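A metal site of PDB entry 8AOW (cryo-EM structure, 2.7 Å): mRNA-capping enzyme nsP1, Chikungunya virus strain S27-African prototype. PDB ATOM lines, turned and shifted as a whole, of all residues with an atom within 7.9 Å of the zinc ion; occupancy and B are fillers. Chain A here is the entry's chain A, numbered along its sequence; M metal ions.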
ATOM      1  N   LEU A  62     -20.773  16.333  -1.952  1.00  0.00           N
ATOM      2  CA  LEU A  62     -20.173  17.281  -2.886  1.00  0.00           C
ATOM      3  C   LEU A  62     -18.663  17.227  -2.753  1.00  0.00           C
ATOM      4  O   LEU A  62     -18.124  17.325  -1.646  1.00  0.00           O
ATOM      5  CB  LEU A  62     -20.677  18.697  -2.614  1.00  0.00           C
ATOM      6  CG  LEU A  62     -22.097  19.045  -3.027  1.00  0.00           C
ATOM      7  CD1 LEU A  62     -22.289  20.550  -3.007  1.00  0.00           C
ATOM      8  CD2 LEU A  62     -22.429  18.474  -4.387  1.00  0.00           C
ATOM      9  N   ASP A  63     -17.974  17.061  -3.873  1.00  0.00           N
ATOM     10  CA  ASP A  63     -16.509  17.082  -3.905  1.00  0.00           C
ATOM     11  C   ASP A  63     -16.116  18.376  -4.594  1.00  0.00           C
ATOM     12  O   ASP A  63     -16.146  18.470  -5.818  1.00  0.00           O
ATOM     13  CB  ASP A  63     -15.955  15.853  -4.616  1.00  0.00           C
ATOM     14  CG  ASP A  63     -14.559  15.499  -4.164  1.00  0.00           C
ATOM     15  OD1 ASP A  63     -14.277  15.628  -2.954  1.00  0.00           O
ATOM     16  OD2 ASP A  63     -13.744  15.068  -5.004  1.00  0.00           O
ATOM     17  N   ILE A  64     -15.760  19.374  -3.778  1.00  0.00           N
ATOM     18  CA  ILE A  64     -15.447  20.701  -4.304  1.00  0.00           C
ATOM     19  C   ILE A  64     -14.032  20.702  -4.847  1.00  0.00           C
ATOM     20  O   ILE A  64     -13.091  20.277  -4.173  1.00  0.00           O
ATOM     21  CB  ILE A  64     -15.626  21.755  -3.207  1.00  0.00           C
ATOM     22  CG1 ILE A  64     -17.027  21.680  -2.585  1.00  0.00           C
ATOM     23  CG2 ILE A  64     -15.375  23.150  -3.772  1.00  0.00           C
ATOM     24  CD1 ILE A  64     -18.151  21.495  -3.583  1.00  0.00           C
ATOM     25  N   HIS A  79     -20.757  13.825  -6.036  1.00  0.00           N
ATOM     26  CA  HIS A  79     -21.012  14.819  -7.073  1.00  0.00           C
ATOM     27  C   HIS A  79     -19.767  15.689  -7.177  1.00  0.00           C
ATOM     28  O   HIS A  79     -19.478  16.468  -6.263  1.00  0.00           O
ATOM     29  CB  HIS A  79     -22.244  15.660  -6.770  1.00  0.00           C
ATOM     30  CG  HIS A  79     -22.480  16.768  -7.740  1.00  0.00           C
ATOM     31  ND1 HIS A  79     -23.271  16.619  -8.862  1.00  0.00           N
ATOM     32  CD2 HIS A  79     -22.021  18.039  -7.769  1.00  0.00           C
ATOM     33  CE1 HIS A  79     -23.301  17.764  -9.529  1.00  0.00           C
ATOM     34  NE2 HIS A  79     -22.543  18.642  -8.895  1.00  0.00           N
ATOM     35  N   CYS A  80     -19.032  15.549  -8.272  1.00  0.00           N
ATOM     36  CA  CYS A  80     -17.745  16.219  -8.429  1.00  0.00           C
ATOM     37  C   CYS A  80     -17.960  17.582  -9.074  1.00  0.00           C
ATOM     38  O   CYS A  80     -18.558  17.666 -10.155  1.00  0.00           O
ATOM     39  CB  CYS A  80     -16.819  15.349  -9.282  1.00  0.00           C
ATOM     40  SG  CYS A  80     -16.394  13.777  -8.510  1.00  0.00           S
ATOM     41  N   VAL A  81     -17.470  18.636  -8.430  1.00  0.00           N
ATOM     42  CA  VAL A  81     -17.601  20.001  -8.929  1.00  0.00           C
ATOM     43  C   VAL A  81     -16.265  20.381  -9.540  1.00  0.00           C
ATOM     44  O   VAL A  81     -15.257  20.513  -8.845  1.00  0.00           O
ATOM     45  CB  VAL A  81     -18.005  20.957  -7.812  1.00  0.00           C
ATOM     46  CG1 VAL A  81     -18.347  22.317  -8.379  1.00  0.00           C
ATOM     47  CG2 VAL A  81     -19.182  20.401  -7.035  1.00  0.00           C
ATOM     48  N   CYS A  82     -16.241  20.561 -10.867  1.00  0.00           N
ATOM     49  CA  CYS A  82     -15.008  20.774 -11.619  1.00  0.00           C
ATOM     50  C   CYS A  82     -15.134  22.015 -12.472  1.00  0.00           C
ATOM     51  O   CYS A  82     -15.507  21.945 -13.655  1.00  0.00           O
ATOM     52  CB  CYS A  82     -14.674  19.552 -12.477  1.00  0.00           C
ATOM     53  SG  CYS A  82     -14.548  18.021 -11.543  1.00  0.00           S
ATOM     54  N   THR A 128     -25.658  21.404 -17.694  1.00  0.00           N
ATOM     55  CA  THR A 128     -26.488  20.396 -17.047  1.00  0.00           C
ATOM     56  C   THR A 128     -25.856  19.955 -15.722  1.00  0.00           C
ATOM     57  O   THR A 128     -24.630  19.912 -15.588  1.00  0.00           O
ATOM     58  CB  THR A 128     -26.702  19.188 -17.973  1.00  0.00           C
ATOM     59  OG1 THR A 128     -27.686  18.322 -17.409  1.00  0.00           O
ATOM     60  CG2 THR A 128     -25.414  18.405 -18.157  1.00  0.00           C
ATOM     61  N   GLU A 129     -26.707  19.660 -14.746  1.00  0.00           N
ATOM     62  CA  GLU A 129     -26.262  19.299 -13.401  1.00  0.00           C
ATOM     63  C   GLU A 129     -26.531  17.809 -13.199  1.00  0.00           C
ATOM     64  O   GLU A 129     -27.593  17.407 -12.722  1.00  0.00           O
ATOM     65  CB  GLU A 129     -26.975  20.143 -12.354  1.00  0.00           C
ATOM     66  CG  GLU A 129     -26.333  20.112 -10.991  1.00  0.00           C
ATOM     67  CD  GLU A 129     -25.168  21.083 -10.866  1.00  0.00           C
ATOM     68  OE1 GLU A 129     -25.315  22.245 -11.262  1.00  0.00           O
ATOM     69  OE2 GLU A 129     -24.098  20.661 -10.379  1.00  0.00           O
ATOM     70  N   THR A 130     -25.570  16.999 -13.575  1.00  0.00           N
ATOM     71  CA  THR A 130     -25.689  15.550 -13.471  1.00  0.00           C
ATOM     72  C   THR A 130     -25.327  15.060 -12.070  1.00  0.00           C
ATOM     73  O   THR A 130     -24.602  15.748 -11.342  1.00  0.00           O
ATOM     74  CB  THR A 130     -24.812  14.882 -14.518  1.00  0.00           C
ATOM     75  OG1 THR A 130     -23.437  15.031 -14.152  1.00  0.00           O
ATOM     76  CG2 THR A 130     -25.064  15.492 -15.892  1.00  0.00           C
ATOM     77  N   PRO A 131     -25.815  13.888 -11.672  1.00  0.00           N
ATOM     78  CA  PRO A 131     -25.594  13.423 -10.286  1.00  0.00           C
ATOM     79  C   PRO A 131     -24.133  13.291  -9.889  1.00  0.00           C
ATOM     80  O   PRO A 131     -23.810  13.510  -8.719  1.00  0.00           O
ATOM     81  CB  PRO A 131     -26.318  12.069 -10.257  1.00  0.00           C
ATOM     82  CG  PRO A 131     -27.331  12.154 -11.325  1.00  0.00           C
ATOM     83  CD  PRO A 131     -26.697  12.964 -12.414  1.00  0.00           C
ATOM     84  N   THR A 132     -23.243  12.929 -10.817  1.00  0.00           N
ATOM     85  CA  THR A 132     -21.861  12.648 -10.445  1.00  0.00           C
ATOM     86  C   THR A 132     -20.842  13.626 -11.018  1.00  0.00           C
ATOM     87  O   THR A 132     -19.657  13.486 -10.714  1.00  0.00           O
ATOM     88  CB  THR A 132     -21.481  11.220 -10.871  1.00  0.00           C
ATOM     89  OG1 THR A 132     -20.977  11.232 -12.205  1.00  0.00           O
ATOM     90  CG2 THR A 132     -22.670  10.300 -10.792  1.00  0.00           C
ATOM     91  N   PHE A 133     -21.258  14.600 -11.819  1.00  0.00           N
ATOM     92  CA  PHE A 133     -20.302  15.505 -12.433  1.00  0.00           C
ATOM     93  C   PHE A 133     -20.989  16.802 -12.831  1.00  0.00           C
ATOM     94  O   PHE A 133     -22.162  16.810 -13.206  1.00  0.00           O
ATOM     95  CB  PHE A 133     -19.641  14.861 -13.661  1.00  0.00           C
ATOM     96  CG  PHE A 133     -18.504  15.663 -14.227  1.00  0.00           C
ATOM     97  CD1 PHE A 133     -17.238  15.564 -13.687  1.00  0.00           C
ATOM     98  CD2 PHE A 133     -18.702  16.512 -15.294  1.00  0.00           C
ATOM     99  CE1 PHE A 133     -16.189  16.298 -14.198  1.00  0.00           C
ATOM    100  CE2 PHE A 133     -17.663  17.256 -15.819  1.00  0.00           C
ATOM    101  CZ  PHE A 133     -16.409  17.138 -15.270  1.00  0.00           C
ATOM    102  N   CYS A 134     -20.240  17.902 -12.735  1.00  0.00           N
ATOM    103  CA  CYS A 134     -20.680  19.195 -13.226  1.00  0.00           C
ATOM    104  C   CYS A 134     -19.451  20.075 -13.433  1.00  0.00           C
ATOM    105  O   CYS A 134     -18.390  19.818 -12.870  1.00  0.00           O
ATOM    106  CB  CYS A 134     -21.660  19.870 -12.254  1.00  0.00           C
ATOM    107  SG  CYS A 134     -20.873  20.684 -10.841  1.00  0.00           S
ATOM    108  N   LEU A 135     -19.625  21.122 -14.240  1.00  0.00           N
ATOM    109  CA  LEU A 135     -18.548  22.045 -14.563  1.00  0.00           C
ATOM    110  C   LEU A 135     -18.719  23.399 -13.877  1.00  0.00           C
ATOM    111  O   LEU A 135     -18.185  24.399 -14.353  1.00  0.00           O
ATOM    112  CB  LEU A 135     -18.449  22.236 -16.077  1.00  0.00           C
ATOM    113  CG  LEU A 135     -18.003  21.039 -16.912  1.00  0.00           C
ATOM    114  CD1 LEU A 135     -18.159  21.346 -18.393  1.00  0.00           C
ATOM    115  CD2 LEU A 135     -16.578  20.640 -16.598  1.00  0.00           C
ATOM    116  N   HIS A 136     -19.459  23.448 -12.780  1.00  0.00           N
ATOM    117  CA  HIS A 136     -19.719  24.683 -12.067  1.00  0.00           C
ATOM    118  C   HIS A 136     -18.680  24.908 -10.978  1.00  0.00           C
ATOM    119  O   HIS A 136     -17.713  24.157 -10.846  1.00  0.00           O
ATOM    120  CB  HIS A 136     -21.135  24.661 -11.483  1.00  0.00           C
ATOM    121  CG  HIS A 136     -22.209  24.647 -12.531  1.00  0.00           C
ATOM    122  ND1 HIS A 136     -22.822  23.484 -12.950  1.00  0.00           N
ATOM    123  CD2 HIS A 136     -22.781  25.654 -13.240  1.00  0.00           C
ATOM    124  CE1 HIS A 136     -23.717  23.774 -13.878  1.00  0.00           C
ATOM    125  NE2 HIS A 136     -23.714  25.086 -14.070  1.00  0.00           N
ATOM    126  N   THR A 137     -18.865  25.953 -10.187  1.00  0.00           N
ATOM    127  CA  THR A 137     -18.017  26.228  -9.039  1.00  0.00           C
ATOM    128  C   THR A 137     -18.765  25.884  -7.747  1.00  0.00           C
ATOM    129  O   THR A 137     -19.893  25.409  -7.761  1.00  0.00           O
ATOM    130  CB  THR A 137     -17.567  27.684  -9.033  1.00  0.00           C
ATOM    131  OG1 THR A 137     -18.704  28.544  -8.899  1.00  0.00           O
ATOM    132  CG2 THR A 137     -16.846  28.028 -10.308  1.00  0.00           C
ATOM    133  N   ASP A 138     -18.099  26.141  -6.626  1.00  0.00           N
ATOM    134  CA  ASP A 138     -18.737  25.911  -5.336  1.00  0.00           C
ATOM    135  C   ASP A 138     -19.920  26.848  -5.114  1.00  0.00           C
ATOM    136  O   ASP A 138     -20.878  26.478  -4.419  1.00  0.00           O
ATOM    137  CB  ASP A 138     -17.713  26.077  -4.206  1.00  0.00           C
ATOM    138  CG  ASP A 138     -17.026  27.426  -4.228  1.00  0.00           C
ATOM    139  OD1 ASP A 138     -17.217  28.179  -5.197  1.00  0.00           O
ATOM    140  OD2 ASP A 138     -16.299  27.730  -3.265  1.00  0.00           O
ATOM    141  N   SER A 140     -21.709  28.274  -7.689  1.00  0.00           N
ATOM    142  CA  SER A 140     -22.631  28.211  -8.810  1.00  0.00           C
ATOM    143  C   SER A 140     -23.199  26.833  -9.067  1.00  0.00           C
ATOM    144  O   SER A 140     -24.112  26.698  -9.891  1.00  0.00           O
ATOM    145  CB  SER A 140     -21.943  28.705 -10.095  1.00  0.00           C
ATOM    146  OG  SER A 140     -21.045  27.739 -10.603  1.00  0.00           O
ATOM    147  N   CYS A 141     -22.703  25.805  -8.388  1.00  0.00           N
ATOM    148  CA  CYS A 141     -23.312  24.483  -8.479  1.00  0.00           C
ATOM    149  C   CYS A 141     -24.692  24.507  -7.826  1.00  0.00           C
ATOM    150  O   CYS A 141     -24.913  25.183  -6.820  1.00  0.00           O
ATOM    151  CB  CYS A 141     -22.426  23.444  -7.805  1.00  0.00           C
ATOM    152  SG  CYS A 141     -23.273  21.915  -7.363  1.00  0.00           S
ATOM    153  N   ARG A 142     -25.626  23.769  -8.424  1.00  0.00           N
ATOM    154  CA  ARG A 142     -26.988  23.712  -7.922  1.00  0.00           C
ATOM    155  C   ARG A 142     -27.328  22.397  -7.226  1.00  0.00           C
ATOM    156  O   ARG A 142     -28.407  22.288  -6.644  1.00  0.00           O
ATOM    157  CB  ARG A 142     -27.986  23.933  -9.065  1.00  0.00           C
ATOM    158  CG  ARG A 142     -27.815  25.248  -9.799  1.00  0.00           C
ATOM    159  CD  ARG A 142     -28.777  25.347 -10.957  1.00  0.00           C
ATOM    160  NE  ARG A 142     -28.200  26.070 -12.089  1.00  0.00           N
ATOM    161  CZ  ARG A 142     -27.696  25.493 -13.162  1.00  0.00           C
ATOM    162  NH1 ARG A 142     -27.694  24.173 -13.310  1.00  0.00           N
ATOM    163  NH2 ARG A 142     -27.182  26.250 -14.128  1.00  0.00           N
ATOM    164  N   GLN A 143     -26.449  21.410  -7.284  1.00  0.00           N
ATOM    165  CA  GLN A 143     -26.723  20.105  -6.691  1.00  0.00           C
ATOM    166  C   GLN A 143     -26.780  20.219  -5.182  1.00  0.00           C
ATOM    167  O   GLN A 143     -25.778  20.554  -4.535  1.00  0.00           O
ATOM    168  CB  GLN A 143     -25.666  19.087  -7.119  1.00  0.00           C
ATOM    169  CG  GLN A 143     -25.880  17.683  -6.556  1.00  0.00           C
ATOM    170  CD  GLN A 143     -27.059  16.962  -7.175  1.00  0.00           C
ATOM    171  OE1 GLN A 143     -28.207  17.387  -7.067  1.00  0.00           O
ATOM    172  NE2 GLN A 143     -26.776  15.842  -7.834  1.00  0.00           N
ATOM    173  N   ARG A 144     -27.947  19.962  -4.605  1.00  0.00           N
ATOM    174  CA  ARG A 144     -28.085  19.902  -3.161  1.00  0.00           C
ATOM    175  C   ARG A 144     -27.463  18.614  -2.637  1.00  0.00           C
ATOM    176  O   ARG A 144     -27.522  17.574  -3.296  1.00  0.00           O
ATOM    177  CB  ARG A 144     -29.567  19.967  -2.788  1.00  0.00           C
ATOM    178  CG  ARG A 144     -30.116  21.370  -2.707  1.00  0.00           C
ATOM    179  CD  ARG A 144     -31.500  21.393  -2.090  1.00  0.00           C
ATOM    180  NE  ARG A 144     -31.685  22.536  -1.215  1.00  0.00           N
ATOM    181  CZ  ARG A 144     -31.735  22.464   0.113  1.00  0.00           C
ATOM    182  NH1 ARG A 144     -31.615  21.311   0.745  1.00  0.00           N
ATOM    183  NH2 ARG A 144     -31.914  23.572   0.818  1.00  0.00           N
ATOM    184  N   LYS A 168     -27.402  25.123   0.615  1.00  0.00           N
ATOM    185  CA  LYS A 168     -27.802  24.005  -0.231  1.00  0.00           C
ATOM    186  C   LYS A 168     -28.098  22.756   0.582  1.00  0.00           C
ATOM    187  O   LYS A 168     -28.198  21.661   0.010  1.00  0.00           O
ATOM    188  CB  LYS A 168     -26.719  23.709  -1.268  1.00  0.00           C
ATOM    189  CG  LYS A 168     -26.849  24.497  -2.547  1.00  0.00           C
ATOM    190  CD  LYS A 168     -26.148  23.785  -3.682  1.00  0.00           C
ATOM    191  CE  LYS A 168     -24.646  23.846  -3.514  1.00  0.00           C
ATOM    192  NZ  LYS A 168     -23.934  23.221  -4.643  1.00  0.00           N
HETATM  193 ZN    ZN M   1     -22.564  20.896  -9.294  1.00  0.00          ZN
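The zinc ion is bound by the side-chain carboxylate of Glu 129 (1.9 Å), a ring nitrogen (NE2) of His 79 (2.3 Å), the side-chain sulfur of Cys 141 (2.3 Å) and the side-chain sulfur of Cys 134 (2.3 Å).
The zinc ion has four donor atoms within binding distance.
The side-chain sulfur (SG) of Cys 134 lies close to the backbone NH (N) of His 136, at 3.7 Å.
O of Thr 130 lies within hydrogen-bond range of ND1 of His 79 (2.9 Å).
The backbone NH (N) of Cys 134 sits at hydrogen-bond distance from the backbone carbonyl oxygen (O) of Cys 80.
N of Asp 63 sits at hydrogen-bond distance from O of His 79 (2.9 Å).
O of Cys 141 is in hydrogen-bond range of NZ of Lys 168, 3.1 Å away.
O of Pro 131 sits at hydrogen-bond distance from ND1 of His 79.
OE1 of Glu 129 is in salt-bridge range of NH1 of Arg 142 (3.7 Å).
The backbone carbonyl oxygen of Cys 134 lies within hydrogen-bond range of the backbone NH of Cys 82 (3.0 Å).
Within 4 Å of the zinc ion: His 79, Glu 129, Cys 134 and Cys 141.
The nearest printed residue that does not touch the zinc ion is Val 81 (4.1 Å).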
